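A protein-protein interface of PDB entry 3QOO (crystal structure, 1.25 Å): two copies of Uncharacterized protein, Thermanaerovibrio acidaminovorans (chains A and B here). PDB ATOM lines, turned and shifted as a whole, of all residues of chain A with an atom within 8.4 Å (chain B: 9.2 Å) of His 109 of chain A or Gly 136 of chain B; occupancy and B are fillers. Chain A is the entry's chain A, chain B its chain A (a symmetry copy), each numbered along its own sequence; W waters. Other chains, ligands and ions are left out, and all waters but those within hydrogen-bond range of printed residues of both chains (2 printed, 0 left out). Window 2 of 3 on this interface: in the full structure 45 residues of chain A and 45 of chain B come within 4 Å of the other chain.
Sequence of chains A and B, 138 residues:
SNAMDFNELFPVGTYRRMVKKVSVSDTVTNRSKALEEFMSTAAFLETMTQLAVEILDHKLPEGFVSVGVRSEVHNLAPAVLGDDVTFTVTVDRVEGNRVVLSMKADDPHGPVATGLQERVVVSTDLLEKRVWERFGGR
The guanidinium group (NE) of Arg 134 of chain B lies close to the backbone carbonyl oxygen (O) of Pro 78 of chain A (3.5 Å). The side-chain carboxylate (OD1) of Asp 107 of chain A lies within salt-bridge range of the guanidinium group (NH2) of Arg 134 of chain B (3.1 Å). The guanidinium group of Arg 138 of chain B lies within hydrogen-bond range of the backbone carbonyl oxygen of Pro 108 of chain A, at 2.9 Å. O of Arg 134 of chain B lies within hydrogen-bond range of ND1 of His 109 of chain A. The guanidinium group of Arg 138 of chain B sits at hydrogen-bond distance from a ring nitrogen (ND1) of His 109 of chain A (3.5 Å). NH2 of Arg 134 of chain B sits at hydrogen-bond distance from O of Gly 110 of chain A.
The backbone NH of Ala 77 of chain A lies within hydrogen-bond range of the backbone carbonyl oxygen of Val 112 of chain A (3.2 Å). OD2 of Asp 83 of chain A lies close to OD2 of Asp 107 of chain A (2.5 Å). N of His 109 of chain A lies within hydrogen-bond range of OD1 of Asp 107 of chain A. OD1 of Asp 107 of chain A is in hydrogen-bond range of N of Gly 110 of chain A (3.2 Å).
Arg 134 of chain B touches Ala 77 of chain A. CD of Pro 78 of chain A touches CZ of Arg 130 of chain B, at 3.7 Å. Pro 78 of chain A touches Val 131 of chain B (CG to CG2, 3.9 Å). O of Pro 78 of chain A touches CE2 of Phe 135 of chain B, at 3.3 Å. Asp 83 of chain A touches Phe 135 of chain B. Asp 107 of chain A touches Phe 135 of chain B (OD2 to CZ, 3.5 Å). CD2 of His 109 of chain A touches CD1 of Phe 135 of chain B, at 3.6 Å. His 109 of chain A touches Gly 136 of chain B. NH2 of Arg 134 of chain B touches O of Pro 111 of chain A (3.6 Å). Arg 134 of chain B touches Val 112 of chain A.
Of the printed residues of chain B, His 109 of chain A touches Arg 134 (3.2 Å), Phe 135 (3.6 Å), Gly 136 (3.9 Å) and Arg 138 (3.5 Å). Gly 136 of chain B touches just one residue of chain A: His 109 (3.9 Å). Of the printed residues of chain B, Pro 108 of chain A touches Arg 138. Of the printed residues of chain B, Val 112 of chain A touches Arg 134. Of the printed residues of chain B, Val 80 of chain A touches Val 131 (3.7 Å) and Phe 135 (3.5 Å). Printed residues of chain A within 4 Å of Arg 134 of chain B: Ala 77 (3.4 Å), Pro 78 (3.3 Å), Asp 107 (3.1 Å), His 109 (3.2 Å), Gly 110 (3.2 Å), Pro 111 (3.6 Å) and Val 112 (3.6 Å). Printed residues of chain A within 4 Å of Val 131 of chain B: Pro 78 (3.9 Å) and Val 80 (3.7 Å).
Of the 12 printed residues of chain A, 10 touch a printed residue of chain B. Hydrophobic or aromatic side chains of chain A that line the printed part of chain B: Ala 77, Pro 78, Val 80, His 109 and Val 112. Along chain A the printed residues that touch a printed residue of chain B span positions 77 to 112. Of the 10 printed residues of chain B, 6 touch a printed residue of chain A. Hydrophobic or aromatic side chains of chain B within 4 Å of the printed part of chain A: Val 131 and Phe 135. Among the printed residues, 19 pairs touch across the chains.
No position is printed for both chains. Of the 19 pairs that touch across the chains among the printed residues, none has its exchanged pair printed and touching as well.
Water W2 lies within hydrogen-bond range of the guanidinium group of Arg 134 of chain B (2.5 Å) and the backbone carbonyl oxygen of Pro 111 of chain A (2.8 Å). Water W1 bridges the backbone carbonyl oxygen of Arg 134 of chain B (2.6 Å) and a ring nitrogen (ND1) of His 109 of chain A (3.3 Å).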
ATOM      1  N   ALA A  77      -8.210  10.698   5.093  1.00  0.00           N
ATOM      2  CA  ALA A  77      -8.307   9.606   4.165  1.00  0.00           C
ATOM      3  C   ALA A  77      -9.000   8.433   4.865  1.00  0.00           C
ATOM      4  O   ALA A  77      -9.000   8.336   6.088  1.00  0.00           O
ATOM      5  CB  ALA A  77      -6.896   9.215   3.643  1.00  0.00           C
ATOM      6  N   PRO A  78      -9.619   7.532   4.071  1.00  0.00           N
ATOM      7  CA  PRO A  78     -10.416   6.493   4.683  1.00  0.00           C
ATOM      8  C   PRO A  78      -9.578   5.404   5.356  1.00  0.00           C
ATOM      9  O   PRO A  78      -8.658   4.865   4.755  1.00  0.00           O
ATOM     10  CB  PRO A  78     -11.242   5.956   3.506  1.00  0.00           C
ATOM     11  CG  PRO A  78     -10.361   6.207   2.292  1.00  0.00           C
ATOM     12  CD  PRO A  78      -9.787   7.573   2.589  1.00  0.00           C
ATOM     13  N   VAL A  80     -10.189   1.859   6.287  1.00  0.00           N
ATOM     14  CA  VAL A  80     -11.179   0.836   5.970  1.00  0.00           C
ATOM     15  C   VAL A  80     -11.319  -0.194   7.109  1.00  0.00           C
ATOM     16  O   VAL A  80     -10.396  -0.433   7.894  1.00  0.00           O
ATOM     17  CB  VAL A  80     -10.719   0.108   4.634  1.00  0.00           C
ATOM     18  CG1 VAL A  80      -9.497  -0.765   4.849  1.00  0.00           C
ATOM     19  CG2 VAL A  80     -11.833  -0.696   3.963  1.00  0.00           C
ATOM     20  N   ASP A  83      -8.425  -2.355   8.756  1.00  0.00           N
ATOM     21  CA  ASP A  83      -7.199  -1.564   8.862  1.00  0.00           C
ATOM     22  C   ASP A  83      -6.762  -1.477  10.297  1.00  0.00           C
ATOM     23  O   ASP A  83      -7.578  -1.541  11.183  1.00  0.00           O
ATOM     24  CB  ASP A  83      -7.512  -0.157   8.383  1.00  0.00           C
ATOM     25  CG  ASP A  83      -6.302   0.685   8.043  1.00  0.00           C
ATOM     26  OD1 ASP A  83      -5.173   0.166   7.869  1.00  0.00           O
ATOM     27  OD2 ASP A  83      -6.518   1.912   7.858  1.00  0.00           O
ATOM     28  N   ASP A  84      -5.454  -1.375  10.509  1.00  0.00           N
ATOM     29  CA  ASP A  84      -4.884  -1.067  11.817  1.00  0.00           C
ATOM     30  C   ASP A  84      -4.400   0.347  11.787  1.00  0.00           C
ATOM     31  O   ASP A  84      -3.508   0.707  11.012  1.00  0.00           O
ATOM     32  CB  ASP A  84      -3.768  -2.029  12.173  1.00  0.00           C
ATOM     33  CG  ASP A  84      -4.321  -3.344  12.564  1.00  0.00           C
ATOM     34  OD1 ASP A  84      -5.045  -3.386  13.569  1.00  0.00           O
ATOM     35  OD2 ASP A  84      -4.046  -4.320  11.878  1.00  0.00           O
ATOM     36  N   ASP A 106      -2.571   7.245  11.752  1.00  0.00           N
ATOM     37  CA  ASP A 106      -1.886   6.794  10.556  1.00  0.00           C
ATOM     38  C   ASP A 106      -2.114   5.303  10.391  1.00  0.00           C
ATOM     39  O   ASP A 106      -2.374   4.571  11.342  1.00  0.00           O
ATOM     40  CB  ASP A 106      -0.373   7.049  10.688  1.00  0.00           C
ATOM     41  CG  ASP A 106      -0.049   8.474  11.066  1.00  0.00           C
ATOM     42  OD1 ASP A 106       0.425   8.720  12.206  1.00  0.00           O
ATOM     43  OD2 ASP A 106      -0.288   9.355  10.247  1.00  0.00           O
ATOM     44  N   ASP A 107      -2.013   4.840   9.171  1.00  0.00           N
ATOM     45  CA  ASP A 107      -1.979   3.429   8.929  1.00  0.00           C
ATOM     46  C   ASP A 107      -0.829   3.175   8.006  1.00  0.00           C
ATOM     47  O   ASP A 107      -0.061   4.087   7.694  1.00  0.00           O
ATOM     48  CB  ASP A 107      -3.349   2.953   8.443  1.00  0.00           C
ATOM     49  CG  ASP A 107      -3.704   3.407   7.015  1.00  0.00           C
ATOM     50  OD1 ASP A 107      -2.813   3.882   6.279  1.00  0.00           O
ATOM     51  OD2 ASP A 107      -4.894   3.325   6.632  1.00  0.00           O
ATOM     52  N   PRO A 108      -0.664   1.926   7.581  1.00  0.00           N
ATOM     53  CA  PRO A 108       0.479   1.605   6.735  1.00  0.00           C
ATOM     54  C   PRO A 108       0.585   2.433   5.445  1.00  0.00           C
ATOM     55  O   PRO A 108       1.667   2.542   4.847  1.00  0.00           O
ATOM     56  CB  PRO A 108       0.227   0.133   6.370  1.00  0.00           C
ATOM     57  CG  PRO A 108      -0.655  -0.376   7.487  1.00  0.00           C
ATOM     58  CD  PRO A 108      -1.518   0.751   7.851  1.00  0.00           C
ATOM     59  N   HIS A 109      -0.533   2.984   4.997  1.00  0.00           N
ATOM     60  CA  HIS A 109      -0.558   3.727   3.766  1.00  0.00           C
ATOM     61  C   HIS A 109      -0.399   5.215   3.949  1.00  0.00           C
ATOM     62  O   HIS A 109      -0.259   5.909   2.984  1.00  0.00           O
ATOM     63  CB  HIS A 109      -1.841   3.421   3.003  1.00  0.00           C
ATOM     64  CG  HIS A 109      -1.956   1.985   2.643  1.00  0.00           C
ATOM     65  ND1 HIS A 109      -1.331   1.455   1.533  1.00  0.00           N
ATOM     66  CD2 HIS A 109      -2.522   0.949   3.291  1.00  0.00           C
ATOM     67  CE1 HIS A 109      -1.553   0.155   1.496  1.00  0.00           C
ATOM     68  NE2 HIS A 109      -2.269  -0.177   2.554  1.00  0.00           N
ATOM     69  N   GLY A 110      -0.372   5.696   5.174  1.00  0.00           N
ATOM     70  CA  GLY A 110      -0.200   7.107   5.472  1.00  0.00           C
ATOM     71  C   GLY A 110      -1.229   7.638   6.467  1.00  0.00           C
ATOM     72  O   GLY A 110      -1.976   6.892   7.079  1.00  0.00           O
ATOM     73  N   PRO A 111      -1.266   8.960   6.637  1.00  0.00           N
ATOM     74  CA  PRO A 111      -2.172   9.589   7.593  1.00  0.00           C
ATOM     75  C   PRO A 111      -3.636   9.436   7.193  1.00  0.00           C
ATOM     76  O   PRO A 111      -3.960   9.564   6.002  1.00  0.00           O
ATOM     77  CB  PRO A 111      -1.763  11.064   7.547  1.00  0.00           C
ATOM     78  CG  PRO A 111      -0.484  11.150   6.851  1.00  0.00           C
ATOM     79  CD  PRO A 111      -0.330   9.927   6.015  1.00  0.00           C
ATOM     80  N   VAL A 112      -4.490   9.198   8.179  1.00  0.00           N
ATOM     81  CA  VAL A 112      -5.910   9.107   7.946  1.00  0.00           C
ATOM     82  C   VAL A 112      -6.708  10.205   8.665  1.00  0.00           C
ATOM     83  O   VAL A 112      -7.814  10.533   8.233  1.00  0.00           O
ATOM     84  CB  VAL A 112      -6.480   7.722   8.258  1.00  0.00           C
ATOM     85  CG1 VAL A 112      -5.935   6.690   7.276  1.00  0.00           C
ATOM     86  CG2 VAL A 112      -6.215   7.277   9.701  1.00  0.00           C
ATOM     87  N   LYS B 129     -13.967   3.574  -5.157  1.00  0.00           N
ATOM     88  CA  LYS B 129     -12.687   3.456  -5.841  1.00  0.00           C
ATOM     89  C   LYS B 129     -11.540   4.041  -5.018  1.00  0.00           C
ATOM     90  O   LYS B 129     -10.445   3.485  -4.998  1.00  0.00           O
ATOM     91  CB  LYS B 129     -12.739   4.069  -7.224  1.00  0.00           C
ATOM     92  CG  LYS B 129     -13.528   3.246  -8.204  1.00  0.00           C
ATOM     93  CD  LYS B 129     -13.298   3.670  -9.631  1.00  0.00           C
ATOM     94  CE  LYS B 129     -14.035   2.736 -10.589  1.00  0.00           C
ATOM     95  NZ  LYS B 129     -14.272   1.402  -9.990  1.00  0.00           N
ATOM     96  N   ARG B 130     -11.776   5.144  -4.319  1.00  0.00           N
ATOM     97  CA  ARG B 130     -10.745   5.715  -3.458  1.00  0.00           C
ATOM     98  C   ARG B 130     -10.299   4.691  -2.429  1.00  0.00           C
ATOM     99  O   ARG B 130      -9.098   4.485  -2.230  1.00  0.00           O
ATOM    100  CB  ARG B 130     -11.241   6.987  -2.750  1.00  0.00           C
ATOM    101  CG  ARG B 130     -10.146   7.688  -1.930  1.00  0.00           C
ATOM    102  CD  ARG B 130     -10.550   8.972  -1.246  1.00  0.00           C
ATOM    103  NE  ARG B 130      -9.397   9.539  -0.541  1.00  0.00           N
ATOM    104  CZ  ARG B 130      -9.464  10.504   0.378  1.00  0.00           C
ATOM    105  NH1 ARG B 130     -10.623  11.058   0.731  1.00  0.00           N
ATOM    106  NH2 ARG B 130      -8.359  10.933   0.959  1.00  0.00           N
ATOM    107  N   VAL B 131     -11.260   4.078  -1.753  1.00  0.00           N
ATOM    108  CA  VAL B 131     -10.980   3.098  -0.712  1.00  0.00           C
ATOM    109  C   VAL B 131     -10.229   1.926  -1.311  1.00  0.00           C
ATOM    110  O   VAL B 131      -9.261   1.436  -0.748  1.00  0.00           O
ATOM    111  CB  VAL B 131     -12.288   2.637  -0.028  1.00  0.00           C
ATOM    112  CG1 VAL B 131     -12.048   1.555   1.003  1.00  0.00           C
ATOM    113  CG2 VAL B 131     -12.988   3.847   0.618  1.00  0.00           C
ATOM    114  N   TRP B 132     -10.676   1.445  -2.460  1.00  0.00           N
ATOM    115  CA  TRP B 132     -10.020   0.325  -3.140  1.00  0.00           C
ATOM    116  C   TRP B 132      -8.570   0.657  -3.447  1.00  0.00           C
ATOM    117  O   TRP B 132      -7.668  -0.138  -3.181  1.00  0.00           O
ATOM    118  CB  TRP B 132     -10.749   0.011  -4.445  1.00  0.00           C
ATOM    119  CG  TRP B 132     -10.066  -1.021  -5.292  1.00  0.00           C
ATOM    120  CD1 TRP B 132      -9.271  -0.816  -6.381  1.00  0.00           C
ATOM    121  CD2 TRP B 132     -10.086  -2.425  -5.061  1.00  0.00           C
ATOM    122  NE1 TRP B 132      -8.807  -2.028  -6.857  1.00  0.00           N
ATOM    123  CE2 TRP B 132      -9.288  -3.027  -6.059  1.00  0.00           C
ATOM    124  CE3 TRP B 132     -10.709  -3.246  -4.107  1.00  0.00           C
ATOM    125  CZ2 TRP B 132      -9.090  -4.403  -6.120  1.00  0.00           C
ATOM    126  CZ3 TRP B 132     -10.511  -4.595  -4.162  1.00  0.00           C
ATOM    127  CH2 TRP B 132      -9.713  -5.170  -5.173  1.00  0.00           C
ATOM    128  N   GLU B 133      -8.334   1.819  -4.049  1.00  0.00           N
ATOM    129  CA  GLU B 133      -6.985   2.191  -4.468  1.00  0.00           C
ATOM    130  C   GLU B 133      -6.054   2.334  -3.255  1.00  0.00           C
ATOM    131  O   GLU B 133      -4.893   1.882  -3.258  1.00  0.00           O
ATOM    132  CB  GLU B 133      -6.992   3.522  -5.223  1.00  0.00           C
ATOM    133  CG  GLU B 133      -7.637   3.449  -6.603  1.00  0.00           C
ATOM    134  CD  GLU B 133      -6.947   2.474  -7.575  1.00  0.00           C
ATOM    135  OE1 GLU B 133      -5.717   2.229  -7.448  1.00  0.00           O
ATOM    136  OE2 GLU B 133      -7.669   1.992  -8.475  1.00  0.00           O
ATOM    137  N   ARG B 134      -6.536   2.999  -2.211  1.00  0.00           N
ATOM    138  CA  ARG B 134      -5.709   3.264  -1.048  1.00  0.00           C
ATOM    139  C   ARG B 134      -5.110   1.969  -0.525  1.00  0.00           C
ATOM    140  O   ARG B 134      -3.900   1.890  -0.251  1.00  0.00           O
ATOM    141  CB  ARG B 134      -6.487   3.978   0.057  1.00  0.00           C
ATOM    142  CG  ARG B 134      -5.653   4.217   1.285  1.00  0.00           C
ATOM    143  CD  ARG B 134      -6.398   5.005   2.344  1.00  0.00           C
ATOM    144  NE  ARG B 134      -5.472   5.212   3.454  1.00  0.00           N
ATOM    145  CZ  ARG B 134      -4.577   6.185   3.492  1.00  0.00           C
ATOM    146  NH1 ARG B 134      -4.491   7.056   2.510  1.00  0.00           N
ATOM    147  NH2 ARG B 134      -3.718   6.256   4.480  1.00  0.00           N
ATOM    148  N   PHE B 135      -5.956   0.949  -0.433  1.00  0.00           N
ATOM    149  CA  PHE B 135      -5.569  -0.328   0.187  1.00  0.00           C
ATOM    150  C   PHE B 135      -5.088  -1.384  -0.779  1.00  0.00           C
ATOM    151  O   PHE B 135      -4.852  -2.521  -0.377  1.00  0.00           O
ATOM    152  CB  PHE B 135      -6.688  -0.820   1.095  1.00  0.00           C
ATOM    153  CG  PHE B 135      -6.851   0.061   2.274  1.00  0.00           C
ATOM    154  CD1 PHE B 135      -6.005  -0.016   3.384  1.00  0.00           C
ATOM    155  CD2 PHE B 135      -7.775   1.087   2.222  1.00  0.00           C
ATOM    156  CE1 PHE B 135      -6.129   0.853   4.423  1.00  0.00           C
ATOM    157  CE2 PHE B 135      -7.917   1.969   3.276  1.00  0.00           C
ATOM    158  CZ  PHE B 135      -7.075   1.855   4.375  1.00  0.00           C
ATOM    159  N   GLY B 136      -4.805  -0.983  -2.002  1.00  0.00           N
ATOM    160  CA  GLY B 136      -4.264  -1.867  -3.004  1.00  0.00           C
ATOM    161  C   GLY B 136      -2.758  -1.905  -2.985  1.00  0.00           C
ATOM    162  O   GLY B 136      -2.110  -1.476  -2.024  1.00  0.00           O
ATOM    163  N   GLY B 137      -2.213  -2.480  -4.055  1.00  0.00           N
ATOM    164  CA  GLY B 137      -0.826  -2.900  -4.110  1.00  0.00           C
ATOM    165  C   GLY B 137       0.080  -1.742  -4.434  1.00  0.00           C
ATOM    166  O   GLY B 137      -0.297  -0.831  -5.185  1.00  0.00           O
ATOM    167  N   ARG B 138       1.279  -1.774  -3.859  1.00  0.00           N
ATOM    168  CA  ARG B 138       2.282  -0.758  -4.142  1.00  0.00           C
ATOM    169  C   ARG B 138       2.876  -1.011  -5.542  1.00  0.00           C
ATOM    170  O   ARG B 138       3.479  -0.118  -6.149  1.00  0.00           O
ATOM    171  CB  ARG B 138       3.366  -0.736  -3.040  1.00  0.00           C
ATOM    172  CG  ARG B 138       3.304   0.500  -2.064  1.00  0.00           C
ATOM    173  CD  ARG B 138       2.556   0.295  -0.710  1.00  0.00           C
ATOM    174  NE  ARG B 138       2.847   1.405   0.224  1.00  0.00           N
ATOM    175  CZ  ARG B 138       2.559   1.435   1.532  1.00  0.00           C
ATOM    176  NH1 ARG B 138       1.952   0.414   2.134  1.00  0.00           N
ATOM    177  NH2 ARG B 138       2.885   2.508   2.254  1.00  0.00           N
ATOM    178  OXT ARG B 138       2.736  -2.101  -6.129  1.00  0.00           O
HETATM  179  O   HOH W   1      -1.829   3.027  -1.377  1.00  0.00           O
HETATM  180  O   HOH W   2      -2.843   8.616   3.635  1.00  0.00           O
